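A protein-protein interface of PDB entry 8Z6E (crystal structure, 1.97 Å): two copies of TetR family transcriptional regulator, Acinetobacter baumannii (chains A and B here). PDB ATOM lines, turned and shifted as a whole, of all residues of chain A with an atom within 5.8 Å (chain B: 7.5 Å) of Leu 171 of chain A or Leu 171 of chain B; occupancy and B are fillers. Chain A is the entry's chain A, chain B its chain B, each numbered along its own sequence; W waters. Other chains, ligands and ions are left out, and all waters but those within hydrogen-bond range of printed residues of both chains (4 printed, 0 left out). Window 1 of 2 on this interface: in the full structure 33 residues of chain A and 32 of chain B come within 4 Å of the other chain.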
ATOM      1  N   TYR A 113       1.247  23.800   0.412  1.00  0.00           N
ATOM      2  CA  TYR A 113       0.309  22.690   0.313  1.00  0.00           C
ATOM      3  C   TYR A 113       0.774  21.658  -0.706  1.00  0.00           C
ATOM      4  O   TYR A 113       1.160  21.992  -1.831  1.00  0.00           O
ATOM      5  CB  TYR A 113      -1.074  23.208  -0.066  1.00  0.00           C
ATOM      6  CG  TYR A 113      -2.149  22.154  -0.056  1.00  0.00           C
ATOM      7  CD1 TYR A 113      -2.629  21.643   1.143  1.00  0.00           C
ATOM      8  CD2 TYR A 113      -2.714  21.695  -1.240  1.00  0.00           C
ATOM      9  CE1 TYR A 113      -3.608  20.691   1.163  1.00  0.00           C
ATOM     10  CE2 TYR A 113      -3.713  20.753  -1.228  1.00  0.00           C
ATOM     11  CZ  TYR A 113      -4.148  20.247  -0.020  1.00  0.00           C
ATOM     12  OH  TYR A 113      -5.147  19.300  -0.009  1.00  0.00           O
ATOM     13  N   GLY A 115      -1.053  18.345  -0.454  1.00  0.00           N
ATOM     14  CA  GLY A 115      -2.041  17.329  -0.169  1.00  0.00           C
ATOM     15  C   GLY A 115      -2.382  17.270   1.315  1.00  0.00           C
ATOM     16  O   GLY A 115      -1.596  17.652   2.186  1.00  0.00           O
ATOM     17  N   THR A 119      -4.749  12.148   2.425  1.00  0.00           N
ATOM     18  CA  THR A 119      -4.331  11.731   1.088  1.00  0.00           C
ATOM     19  C   THR A 119      -2.924  11.183   1.138  1.00  0.00           C
ATOM     20  O   THR A 119      -2.644  10.129   0.554  1.00  0.00           O
ATOM     21  CB  THR A 119      -4.428  12.895   0.096  1.00  0.00           C
ATOM     22  OG1 THR A 119      -5.803  13.232  -0.073  1.00  0.00           O
ATOM     23  CG2 THR A 119      -3.853  12.503  -1.287  1.00  0.00           C
ATOM     24  N   ASN A 139     -14.405   9.649   3.972  1.00  0.00           N
ATOM     25  CA  ASN A 139     -14.954  10.299   2.792  1.00  0.00           C
ATOM     26  C   ASN A 139     -16.425   9.959   2.580  1.00  0.00           C
ATOM     27  O   ASN A 139     -17.189  10.823   2.149  1.00  0.00           O
ATOM     28  CB  ASN A 139     -14.120   9.945   1.569  1.00  0.00           C
ATOM     29  CG  ASN A 139     -12.811  10.695   1.536  1.00  0.00           C
ATOM     30  OD1 ASN A 139     -12.715  11.793   2.074  1.00  0.00           O
ATOM     31  ND2 ASN A 139     -11.796  10.112   0.903  1.00  0.00           N
ATOM     32  N   ASN A 167     -13.484  17.781  -3.386  1.00  0.00           N
ATOM     33  CA  ASN A 167     -12.330  16.903  -3.321  1.00  0.00           C
ATOM     34  C   ASN A 167     -11.280  17.267  -4.367  1.00  0.00           C
ATOM     35  O   ASN A 167     -10.088  17.067  -4.131  1.00  0.00           O
ATOM     36  CB  ASN A 167     -12.779  15.446  -3.472  1.00  0.00           C
ATOM     37  CG  ASN A 167     -13.481  14.918  -2.221  1.00  0.00           C
ATOM     38  OD1 ASN A 167     -13.136  15.296  -1.095  1.00  0.00           O
ATOM     39  ND2 ASN A 167     -14.479  14.053  -2.416  1.00  0.00           N
ATOM     40  N   GLY A 168     -11.688  17.830  -5.511  1.00  0.00           N
ATOM     41  CA  GLY A 168     -10.706  18.279  -6.487  1.00  0.00           C
ATOM     42  C   GLY A 168      -9.922  19.503  -6.043  1.00  0.00           C
ATOM     43  O   GLY A 168      -8.761  19.674  -6.425  1.00  0.00           O
ATOM     44  N   ILE A 169     -10.529  20.359  -5.219  1.00  0.00           N
ATOM     45  CA  ILE A 169      -9.794  21.456  -4.588  1.00  0.00           C
ATOM     46  C   ILE A 169      -8.666  20.912  -3.706  1.00  0.00           C
ATOM     47  O   ILE A 169      -7.642  21.578  -3.504  1.00  0.00           O
ATOM     48  CB  ILE A 169     -10.789  22.331  -3.786  1.00  0.00           C
ATOM     49  CG1 ILE A 169     -11.715  23.085  -4.744  1.00  0.00           C
ATOM     50  CG2 ILE A 169     -10.076  23.296  -2.842  1.00  0.00           C
ATOM     51  CD1 ILE A 169     -12.789  23.922  -4.019  1.00  0.00           C
ATOM     52  N   LEU A 170      -8.830  19.700  -3.184  1.00  0.00           N
ATOM     53  CA  LEU A 170      -7.850  19.070  -2.298  1.00  0.00           C
ATOM     54  C   LEU A 170      -6.729  18.349  -3.047  1.00  0.00           C
ATOM     55  O   LEU A 170      -5.699  18.037  -2.443  1.00  0.00           O
ATOM     56  CB  LEU A 170      -8.539  18.066  -1.378  1.00  0.00           C
ATOM     57  CG  LEU A 170      -9.688  18.590  -0.498  1.00  0.00           C
ATOM     58  CD1 LEU A 170     -10.179  17.480   0.373  1.00  0.00           C
ATOM     59  CD2 LEU A 170      -9.252  19.768   0.321  1.00  0.00           C
ATOM     60  N   LEU A 171      -6.898  18.067  -4.314  1.00  0.00           N
ATOM     61  CA  LEU A 171      -5.820  17.469  -5.086  1.00  0.00           C
ATOM     62  C   LEU A 171      -4.662  18.455  -5.195  1.00  0.00           C
ATOM     63  O   LEU A 171      -4.862  19.597  -5.597  1.00  0.00           O
ATOM     64  CB  LEU A 171      -6.331  17.077  -6.458  1.00  0.00           C
ATOM     65  CG  LEU A 171      -5.498  16.050  -7.220  1.00  0.00           C
ATOM     66  CD1 LEU A 171      -5.866  14.607  -6.823  1.00  0.00           C
ATOM     67  CD2 LEU A 171      -5.694  16.276  -8.684  1.00  0.00           C
ATOM     68  N   PRO A 172      -3.448  18.076  -4.820  1.00  0.00           N
ATOM     69  CA  PRO A 172      -2.346  19.034  -4.893  1.00  0.00           C
ATOM     70  C   PRO A 172      -2.029  19.346  -6.347  1.00  0.00           C
ATOM     71  O   PRO A 172      -2.353  18.576  -7.252  1.00  0.00           O
ATOM     72  CB  PRO A 172      -1.194  18.307  -4.180  1.00  0.00           C
ATOM     73  CG  PRO A 172      -1.516  16.871  -4.341  1.00  0.00           C
ATOM     74  CD  PRO A 172      -3.017  16.775  -4.288  1.00  0.00           C
ATOM     75  N   ALA A 173      -1.444  20.522  -6.559  1.00  0.00           N
ATOM     76  CA  ALA A 173      -1.082  21.037  -7.881  1.00  0.00           C
ATOM     77  C   ALA A 173      -2.294  21.249  -8.771  1.00  0.00           C
ATOM     78  O   ALA A 173      -2.166  21.347  -9.994  1.00  0.00           O
ATOM     79  CB  ALA A 173      -0.066  20.135  -8.593  1.00  0.00           C
ATOM     80  N   SER A 174      -3.475  21.331  -8.175  1.00  0.00           N
ATOM     81  CA  SER A 174      -4.678  21.566  -8.940  1.00  0.00           C
ATOM     82  C   SER A 174      -4.824  23.051  -9.246  1.00  0.00           C
ATOM     83  O   SER A 174      -4.290  23.914  -8.547  1.00  0.00           O
ATOM     84  CB  SER A 174      -5.891  21.012  -8.195  1.00  0.00           C
ATOM     85  OG  SER A 174      -6.515  22.033  -7.450  1.00  0.00           O
ATOM     86  N   ALA B 108      -8.572   6.445 -12.737  1.00  0.00           N
ATOM     87  CA  ALA B 108      -8.764   6.158 -11.326  1.00  0.00           C
ATOM     88  C   ALA B 108      -9.039   4.683 -11.087  1.00  0.00           C
ATOM     89  O   ALA B 108      -8.571   4.121 -10.096  1.00  0.00           O
ATOM     90  CB  ALA B 108      -9.902   7.014 -10.761  1.00  0.00           C
ATOM     91  N   TYR B 113      -4.937   1.233  -7.897  1.00  0.00           N
ATOM     92  CA  TYR B 113      -4.866   2.685  -7.808  1.00  0.00           C
ATOM     93  C   TYR B 113      -4.982   3.210  -6.383  1.00  0.00           C
ATOM     94  O   TYR B 113      -6.045   3.133  -5.754  1.00  0.00           O
ATOM     95  CB  TYR B 113      -5.949   3.281  -8.683  1.00  0.00           C
ATOM     96  CG  TYR B 113      -5.922   4.771  -8.750  1.00  0.00           C
ATOM     97  CD1 TYR B 113      -5.121   5.450  -9.667  1.00  0.00           C
ATOM     98  CD2 TYR B 113      -6.749   5.509  -7.910  1.00  0.00           C
ATOM     99  CE1 TYR B 113      -5.145   6.856  -9.716  1.00  0.00           C
ATOM    100  CE2 TYR B 113      -6.782   6.872  -7.946  1.00  0.00           C
ATOM    101  CZ  TYR B 113      -5.991   7.553  -8.843  1.00  0.00           C
ATOM    102  OH  TYR B 113      -6.078   8.943  -8.834  1.00  0.00           O
ATOM    103  N   ASN B 114      -3.893   3.800  -5.909  1.00  0.00           N
ATOM    104  CA  ASN B 114      -3.842   4.596  -4.697  1.00  0.00           C
ATOM    105  C   ASN B 114      -3.464   6.033  -5.025  1.00  0.00           C
ATOM    106  O   ASN B 114      -2.729   6.685  -4.292  1.00  0.00           O
ATOM    107  CB  ASN B 114      -2.865   3.984  -3.697  1.00  0.00           C
ATOM    108  CG  ASN B 114      -1.407   4.174  -4.108  1.00  0.00           C
ATOM    109  OD1 ASN B 114      -1.078   4.159  -5.306  1.00  0.00           O
ATOM    110  ND2 ASN B 114      -0.519   4.295  -3.115  1.00  0.00           N
ATOM    111  N   GLY B 115      -3.953   6.549  -6.131  1.00  0.00           N
ATOM    112  CA  GLY B 115      -3.542   7.897  -6.459  1.00  0.00           C
ATOM    113  C   GLY B 115      -2.614   7.917  -7.660  1.00  0.00           C
ATOM    114  O   GLY B 115      -1.838   6.982  -7.899  1.00  0.00           O
ATOM    115  N   THR B 116      -2.684   9.005  -8.420  1.00  0.00           N
ATOM    116  CA  THR B 116      -1.918   9.076  -9.651  1.00  0.00           C
ATOM    117  C   THR B 116      -0.440   9.298  -9.364  1.00  0.00           C
ATOM    118  O   THR B 116      -0.040   9.725  -8.277  1.00  0.00           O
ATOM    119  CB  THR B 116      -2.446  10.178 -10.555  1.00  0.00           C
ATOM    120  OG1 THR B 116      -2.025  11.450 -10.042  1.00  0.00           O
ATOM    121  CG2 THR B 116      -3.940  10.115 -10.687  1.00  0.00           C
ATOM    122  N   THR B 119       0.299  12.948  -8.592  1.00  0.00           N
ATOM    123  CA  THR B 119      -0.010  13.299  -7.203  1.00  0.00           C
ATOM    124  C   THR B 119       1.051  12.761  -6.253  1.00  0.00           C
ATOM    125  O   THR B 119       1.467  13.460  -5.325  1.00  0.00           O
ATOM    126  CB  THR B 119      -1.385  12.759  -6.803  1.00  0.00           C
ATOM    127  OG1 THR B 119      -2.386  13.380  -7.608  1.00  0.00           O
ATOM    128  CG2 THR B 119      -1.693  13.044  -5.317  1.00  0.00           C
ATOM    129  N   VAL B 122       4.061  15.111  -6.340  1.00  0.00           N
ATOM    130  CA  VAL B 122       3.875  16.380  -5.637  1.00  0.00           C
ATOM    131  C   VAL B 122       3.952  16.172  -4.125  1.00  0.00           C
ATOM    132  O   VAL B 122       4.546  16.979  -3.397  1.00  0.00           O
ATOM    133  CB  VAL B 122       2.545  17.035  -6.061  1.00  0.00           C
ATOM    134  CG1 VAL B 122       2.262  18.286  -5.227  1.00  0.00           C
ATOM    135  CG2 VAL B 122       2.581  17.387  -7.518  1.00  0.00           C
ATOM    136  N   LYS B 132       6.123  20.313  -8.589  1.00  0.00           N
ATOM    137  CA  LYS B 132       4.798  20.883  -8.412  1.00  0.00           C
ATOM    138  C   LYS B 132       4.435  21.798  -9.578  1.00  0.00           C
ATOM    139  O   LYS B 132       3.282  21.823 -10.024  1.00  0.00           O
ATOM    140  CB  LYS B 132       4.743  21.628  -7.085  1.00  0.00           C
ATOM    141  CG  LYS B 132       3.431  22.307  -6.788  1.00  0.00           C
ATOM    142  CD  LYS B 132       3.630  23.370  -5.712  1.00  0.00           C
ATOM    143  CE  LYS B 132       2.679  23.146  -4.558  1.00  0.00           C
ATOM    144  NZ  LYS B 132       1.362  22.680  -5.059  1.00  0.00           N
ATOM    145  N   VAL B 135       3.474  19.722 -12.569  1.00  0.00           N
ATOM    146  CA  VAL B 135       2.171  19.074 -12.441  1.00  0.00           C
ATOM    147  C   VAL B 135       1.052  20.107 -12.535  1.00  0.00           C
ATOM    148  O   VAL B 135       0.000  19.845 -13.136  1.00  0.00           O
ATOM    149  CB  VAL B 135       2.101  18.239 -11.151  1.00  0.00           C
ATOM    150  CG1 VAL B 135       0.699  17.654 -10.962  1.00  0.00           C
ATOM    151  CG2 VAL B 135       3.096  17.096 -11.229  1.00  0.00           C
ATOM    152  N   ASN B 139      -2.105  20.204 -15.243  1.00  0.00           N
ATOM    153  CA  ASN B 139      -3.514  20.400 -14.896  1.00  0.00           C
ATOM    154  C   ASN B 139      -4.084  21.617 -15.594  1.00  0.00           C
ATOM    155  O   ASN B 139      -5.265  21.633 -15.957  1.00  0.00           O
ATOM    156  CB  ASN B 139      -3.679  20.545 -13.392  1.00  0.00           C
ATOM    157  CG  ASN B 139      -3.597  19.226 -12.682  1.00  0.00           C
ATOM    158  OD1 ASN B 139      -4.130  18.223 -13.162  1.00  0.00           O
ATOM    159  ND2 ASN B 139      -2.904  19.201 -11.548  1.00  0.00           N
ATOM    160  N   LYS B 142      -4.790  20.522 -18.997  1.00  0.00           N
ATOM    161  CA  LYS B 142      -5.922  19.612 -19.111  1.00  0.00           C
ATOM    162  C   LYS B 142      -7.239  20.367 -19.047  1.00  0.00           C
ATOM    163  O   LYS B 142      -8.181  20.040 -19.777  1.00  0.00           O
ATOM    164  CB  LYS B 142      -5.854  18.557 -18.014  1.00  0.00           C
ATOM    165  CG  LYS B 142      -7.039  17.637 -18.006  1.00  0.00           C
ATOM    166  CD  LYS B 142      -6.809  16.490 -17.057  1.00  0.00           C
ATOM    167  CE  LYS B 142      -6.690  16.977 -15.626  1.00  0.00           C
ATOM    168  NZ  LYS B 142      -7.111  15.849 -14.793  1.00  0.00           N
ATOM    169  N   SER B 164     -12.970  20.194 -11.914  1.00  0.00           N
ATOM    170  CA  SER B 164     -12.618  19.901 -10.530  1.00  0.00           C
ATOM    171  C   SER B 164     -13.330  18.650 -10.036  1.00  0.00           C
ATOM    172  O   SER B 164     -12.759  17.886  -9.254  1.00  0.00           O
ATOM    173  CB  SER B 164     -12.927  21.111  -9.653  1.00  0.00           C
ATOM    174  OG  SER B 164     -12.500  20.936  -8.304  1.00  0.00           O
ATOM    175  N   ALA B 165     -14.554  18.397 -10.502  1.00  0.00           N
ATOM    176  CA  ALA B 165     -15.210  17.142 -10.143  1.00  0.00           C
ATOM    177  C   ALA B 165     -14.484  15.945 -10.749  1.00  0.00           C
ATOM    178  O   ALA B 165     -14.390  14.884 -10.118  1.00  0.00           O
ATOM    179  CB  ALA B 165     -16.665  17.155 -10.592  1.00  0.00           C
ATOM    180  N   MET B 166     -13.986  16.073 -11.984  1.00  0.00           N
ATOM    181  CA  MET B 166     -13.146  14.997 -12.501  1.00  0.00           C
ATOM    182  C   MET B 166     -11.837  14.867 -11.751  1.00  0.00           C
ATOM    183  O   MET B 166     -11.338  13.749 -11.574  1.00  0.00           O
ATOM    184  CB  MET B 166     -12.877  15.118 -13.996  1.00  0.00           C
ATOM    185  CG  MET B 166     -14.007  15.384 -14.917  1.00  0.00           C
ATOM    186  SD  MET B 166     -15.082  13.903 -14.933  1.00  0.00           S
ATOM    187  CE  MET B 166     -16.216  14.122 -13.535  1.00  0.00           C
ATOM    188  N   ASN B 167     -11.241  15.974 -11.312  1.00  0.00           N
ATOM    189  CA  ASN B 167     -10.041  15.798 -10.495  1.00  0.00           C
ATOM    190  C   ASN B 167     -10.358  15.158  -9.143  1.00  0.00           C
ATOM    191  O   ASN B 167      -9.499  14.484  -8.575  1.00  0.00           O
ATOM    192  CB  ASN B 167      -9.305  17.125 -10.320  1.00  0.00           C
ATOM    193  CG  ASN B 167      -8.446  17.453 -11.515  1.00  0.00           C
ATOM    194  OD1 ASN B 167      -7.887  16.553 -12.161  1.00  0.00           O
ATOM    195  ND2 ASN B 167      -8.342  18.731 -11.837  1.00  0.00           N
ATOM    196  N   GLY B 168     -11.573  15.318  -8.619  1.00  0.00           N
ATOM    197  CA  GLY B 168     -11.903  14.654  -7.363  1.00  0.00           C
ATOM    198  C   GLY B 168     -11.997  13.152  -7.508  1.00  0.00           C
ATOM    199  O   GLY B 168     -11.668  12.406  -6.580  1.00  0.00           O
ATOM    200  N   ILE B 169     -12.436  12.685  -8.674  1.00  0.00           N
ATOM    201  CA  ILE B 169     -12.401  11.257  -8.972  1.00  0.00           C
ATOM    202  C   ILE B 169     -10.991  10.686  -8.802  1.00  0.00           C
ATOM    203  O   ILE B 169     -10.824   9.513  -8.442  1.00  0.00           O
ATOM    204  CB  ILE B 169     -12.965  11.040 -10.391  1.00  0.00           C
ATOM    205  CG1 ILE B 169     -14.472  11.354 -10.397  1.00  0.00           C
ATOM    206  CG2 ILE B 169     -12.726   9.632 -10.907  1.00  0.00           C
ATOM    207  CD1 ILE B 169     -15.105  11.112 -11.727  1.00  0.00           C
ATOM    208  N   LEU B 170      -9.959  11.493  -9.047  1.00  0.00           N
ATOM    209  CA  LEU B 170      -8.586  11.002  -8.940  1.00  0.00           C
ATOM    210  C   LEU B 170      -8.035  11.044  -7.516  1.00  0.00           C
ATOM    211  O   LEU B 170      -6.939  10.534  -7.276  1.00  0.00           O
ATOM    212  CB  LEU B 170      -7.653  11.795  -9.856  1.00  0.00           C
ATOM    213  CG  LEU B 170      -7.986  11.882 -11.352  1.00  0.00           C
ATOM    214  CD1 LEU B 170      -7.062  12.878 -12.017  1.00  0.00           C
ATOM    215  CD2 LEU B 170      -7.845  10.535 -12.009  1.00  0.00           C
ATOM    216  N   LEU B 171      -8.730  11.660  -6.575  1.00  0.00           N
ATOM    217  CA  LEU B 171      -8.278  11.605  -5.196  1.00  0.00           C
ATOM    218  C   LEU B 171      -8.315  10.153  -4.736  1.00  0.00           C
ATOM    219  O   LEU B 171      -9.257   9.422  -5.079  1.00  0.00           O
ATOM    220  CB  LEU B 171      -9.153  12.498  -4.315  1.00  0.00           C
ATOM    221  CG  LEU B 171      -8.560  13.027  -3.002  1.00  0.00           C
ATOM    222  CD1 LEU B 171      -7.406  14.012  -3.247  1.00  0.00           C
ATOM    223  CD2 LEU B 171      -9.668  13.656  -2.157  1.00  0.00           C
ATOM    224  N   PRO B 172      -7.269   9.661  -4.088  1.00  0.00           N
ATOM    225  CA  PRO B 172      -7.315   8.280  -3.605  1.00  0.00           C
ATOM    226  C   PRO B 172      -8.387   8.138  -2.538  1.00  0.00           C
ATOM    227  O   PRO B 172      -8.722   9.093  -1.830  1.00  0.00           O
ATOM    228  CB  PRO B 172      -5.903   8.036  -3.052  1.00  0.00           C
ATOM    229  CG  PRO B 172      -5.320   9.403  -2.833  1.00  0.00           C
ATOM    230  CD  PRO B 172      -5.955  10.290  -3.877  1.00  0.00           C
ATOM    231  N   ALA B 173      -8.972   6.941  -2.487  1.00  0.00           N
ATOM    232  CA  ALA B 173     -10.091   6.600  -1.615  1.00  0.00           C
ATOM    233  C   ALA B 173     -11.320   7.491  -1.855  1.00  0.00           C
ATOM    234  O   ALA B 173     -12.174   7.606  -0.984  1.00  0.00           O
ATOM    235  CB  ALA B 173      -9.663   6.630  -0.142  1.00  0.00           C
ATOM    236  N   SER B 174     -11.435   8.113  -3.037  1.00  0.00           N
ATOM    237  CA  SER B 174     -12.639   8.869  -3.374  1.00  0.00           C
ATOM    238  C   SER B 174     -13.832   7.925  -3.437  1.00  0.00           C
ATOM    239  O   SER B 174     -13.709   6.769  -3.856  1.00  0.00           O
ATOM    240  CB  SER B 174     -12.471   9.593  -4.723  1.00  0.00           C
ATOM    241  OG  SER B 174     -12.170   8.674  -5.794  1.00  0.00           O
ATOM    242  N   THR B 175     -14.997   8.417  -3.030  1.00  0.00           N
ATOM    243  CA  THR B 175     -16.197   7.590  -3.015  1.00  0.00           C
ATOM    244  C   THR B 175     -17.381   8.447  -3.472  1.00  0.00           C
ATOM    245  O   THR B 175     -17.245   9.649  -3.705  1.00  0.00           O
ATOM    246  CB  THR B 175     -16.405   6.989  -1.617  1.00  0.00           C
ATOM    247  OG1 THR B 175     -17.557   6.132  -1.624  1.00  0.00           O
ATOM    248  CG2 THR B 175     -16.617   8.118  -0.597  1.00  0.00           C
ATOM    249  N   LEU B 177     -18.837   8.579  -6.319  1.00  0.00           N
ATOM    250  CA  LEU B 177     -18.357   9.241  -7.524  1.00  0.00           C
ATOM    251  C   LEU B 177     -19.504   9.738  -8.402  1.00  0.00           C
ATOM    252  O   LEU B 177     -20.496   9.033  -8.595  1.00  0.00           O
ATOM    253  CB  LEU B 177     -17.481   8.293  -8.330  1.00  0.00           C
ATOM    254  CG  LEU B 177     -16.146   8.028  -7.631  1.00  0.00           C
ATOM    255  CD1 LEU B 177     -15.196   7.256  -8.567  1.00  0.00           C
ATOM    256  CD2 LEU B 177     -15.525   9.316  -7.147  1.00  0.00           C
HETATM  257  O   HOH W   1      -1.347  22.133  -4.554  1.00  0.00           O
HETATM  258  O   HOH W   2     -14.290  12.433  -4.906  1.00  0.00           O
HETATM  259  O   HOH W   3      -7.565  11.419   0.315  1.00  0.00           O
HETATM  260  O   HOH W   4     -14.691  10.826  -2.130  1.00  0.00           O
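Among the printed residues, merely in contact across the chains: Thr 119 of chain A with Leu 171 of chain B, Thr 119 of chain A with Pro 172 of chain B, Asn 139 of chain A with Thr 175 of chain B, Asn 167 of chain A with Leu 171 of chain B, Gly 168 of chain A with Ser 164 of chain B, Gly 168 of chain A with Gly 168 of chain B, Ile 169 of chain A with Ser 164 of chain B, Leu 171 of chain A with Thr 119 of chain B, Leu 171 of chain A with Leu 171 of chain B, Pro 172 of chain A with Thr 119 of chain B, Pro 172 of chain A with Val 122 of chain B, Ala 173 of chain A with Val 122 of chain B, Ala 173 of chain A with Lys 132 of chain B, Ala 173 of chain A with Val 135 of chain B and Ser 174 of chain A with Asn 139 of chain B.
Water W3 bridges OG1 of Thr 119 of chain A and O of Pro 172 of chain B. Water W1 lies within hydrogen-bond range of the backbone NH (N) of Ala 173 of chain A (2.6 Å) and the side-chain amino group (NZ) of Lys 132 of chain B (2.8 Å). Water W4 bridges the backbone NH of Thr 175 of chain B and the side-chain amide nitrogen of Asn 167 of chain A. Water W2 bridges the side-chain amide nitrogen (ND2) of Asn 167 of chain A and the backbone carbonyl oxygen (O) of Gly 168 of chain B.
The backbone carbonyl oxygen (O) of Leu 170 of chain A is in hydrogen-bond range of the side-chain hydroxyl (OH) of Tyr 113 of chain A, at 2.8 Å. OG of Ser 174 of chain A is in hydrogen-bond range of O of Gly 168 of chain A, at 3.4 Å. The backbone carbonyl oxygen (O) of Leu 171 of chain A sits close to the side-chain hydroxyl (OG) of Ser 174 of chain A, at 3.5 Å. The backbone NH (N) of Thr 119 of chain B is in hydrogen-bond range of the side-chain hydroxyl (OG1) of Thr 116 of chain B, 3.1 Å away. ND2 of Asn 139 of chain B lies within hydrogen-bond range of O of Val 135 of chain B, 3.4 Å away. The side-chain hydroxyl (OG) of Ser 174 of chain B is in hydrogen-bond range of the backbone carbonyl oxygen (O) of Leu 171 of chain B (3.1 Å).
Gly 115 of chain A touches none of the printed residues of chain B. Of the printed residues of chain B, Thr 119 of chain A touches Leu 171 (3.6 Å) and Pro 172 (3.8 Å). Of the printed residues of chain B, Gly 168 of chain A touches Ser 164 (3.5 Å) and Gly 168 (3.7 Å). Of the printed residues of chain B, Leu 171 of chain A touches Thr 119 and Leu 171. Of chain A, only Thr 119 (3.6 Å), Asn 167 (3.8 Å) and Leu 171 (3.9 Å) come within 4 Å of Leu 171 of chain B. The nearest residue of chain B that does not touch Leu 171 of chain A is Asn 167 of chain B (4.04 Å). The nearest residue of chain A that does not touch Leu 171 of chain B is Leu 170 of chain A (4.4 Å). The nearest printed residue of chain A that does not touch Ala 173 of chain B is Asn 167 of chain A (7.0 Å).
Thr 119 of chain A touches Pro 172 of chain B, and with the chains exchanged Pro 172 of chain A touches Thr 119 of chain B. Asn 167 of chain A touches Leu 171 of chain B, but with the chains exchanged Leu 171 of chain A does not touch Asn 167 of chain B (4.04 Å). Gly 168 of chain A touches its own counterpart, Gly 168 of chain B. Leu 171 of chain A touches its own counterpart, Leu 171 of chain B. Positions printed for both chains: 113, 115, 119, 139, 167, 168, 169, 170, 171, 172, 173 and 174.
The side-chain amide nitrogen (ND2) of Asn 139 of chain A lies within hydrogen-bond range of the backbone carbonyl oxygen (O) of Ala 173 of chain B (3.2 Å). The backbone carbonyl oxygen (O) of Tyr 113 of chain A is in hydrogen-bond range of the side-chain amino group (NZ) of Lys 132 of chain B (3.3 Å). The backbone carbonyl oxygen of Ala 173 of chain A lies within hydrogen-bond range of the side-chain amide nitrogen of Asn 139 of chain B (2.8 Å).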
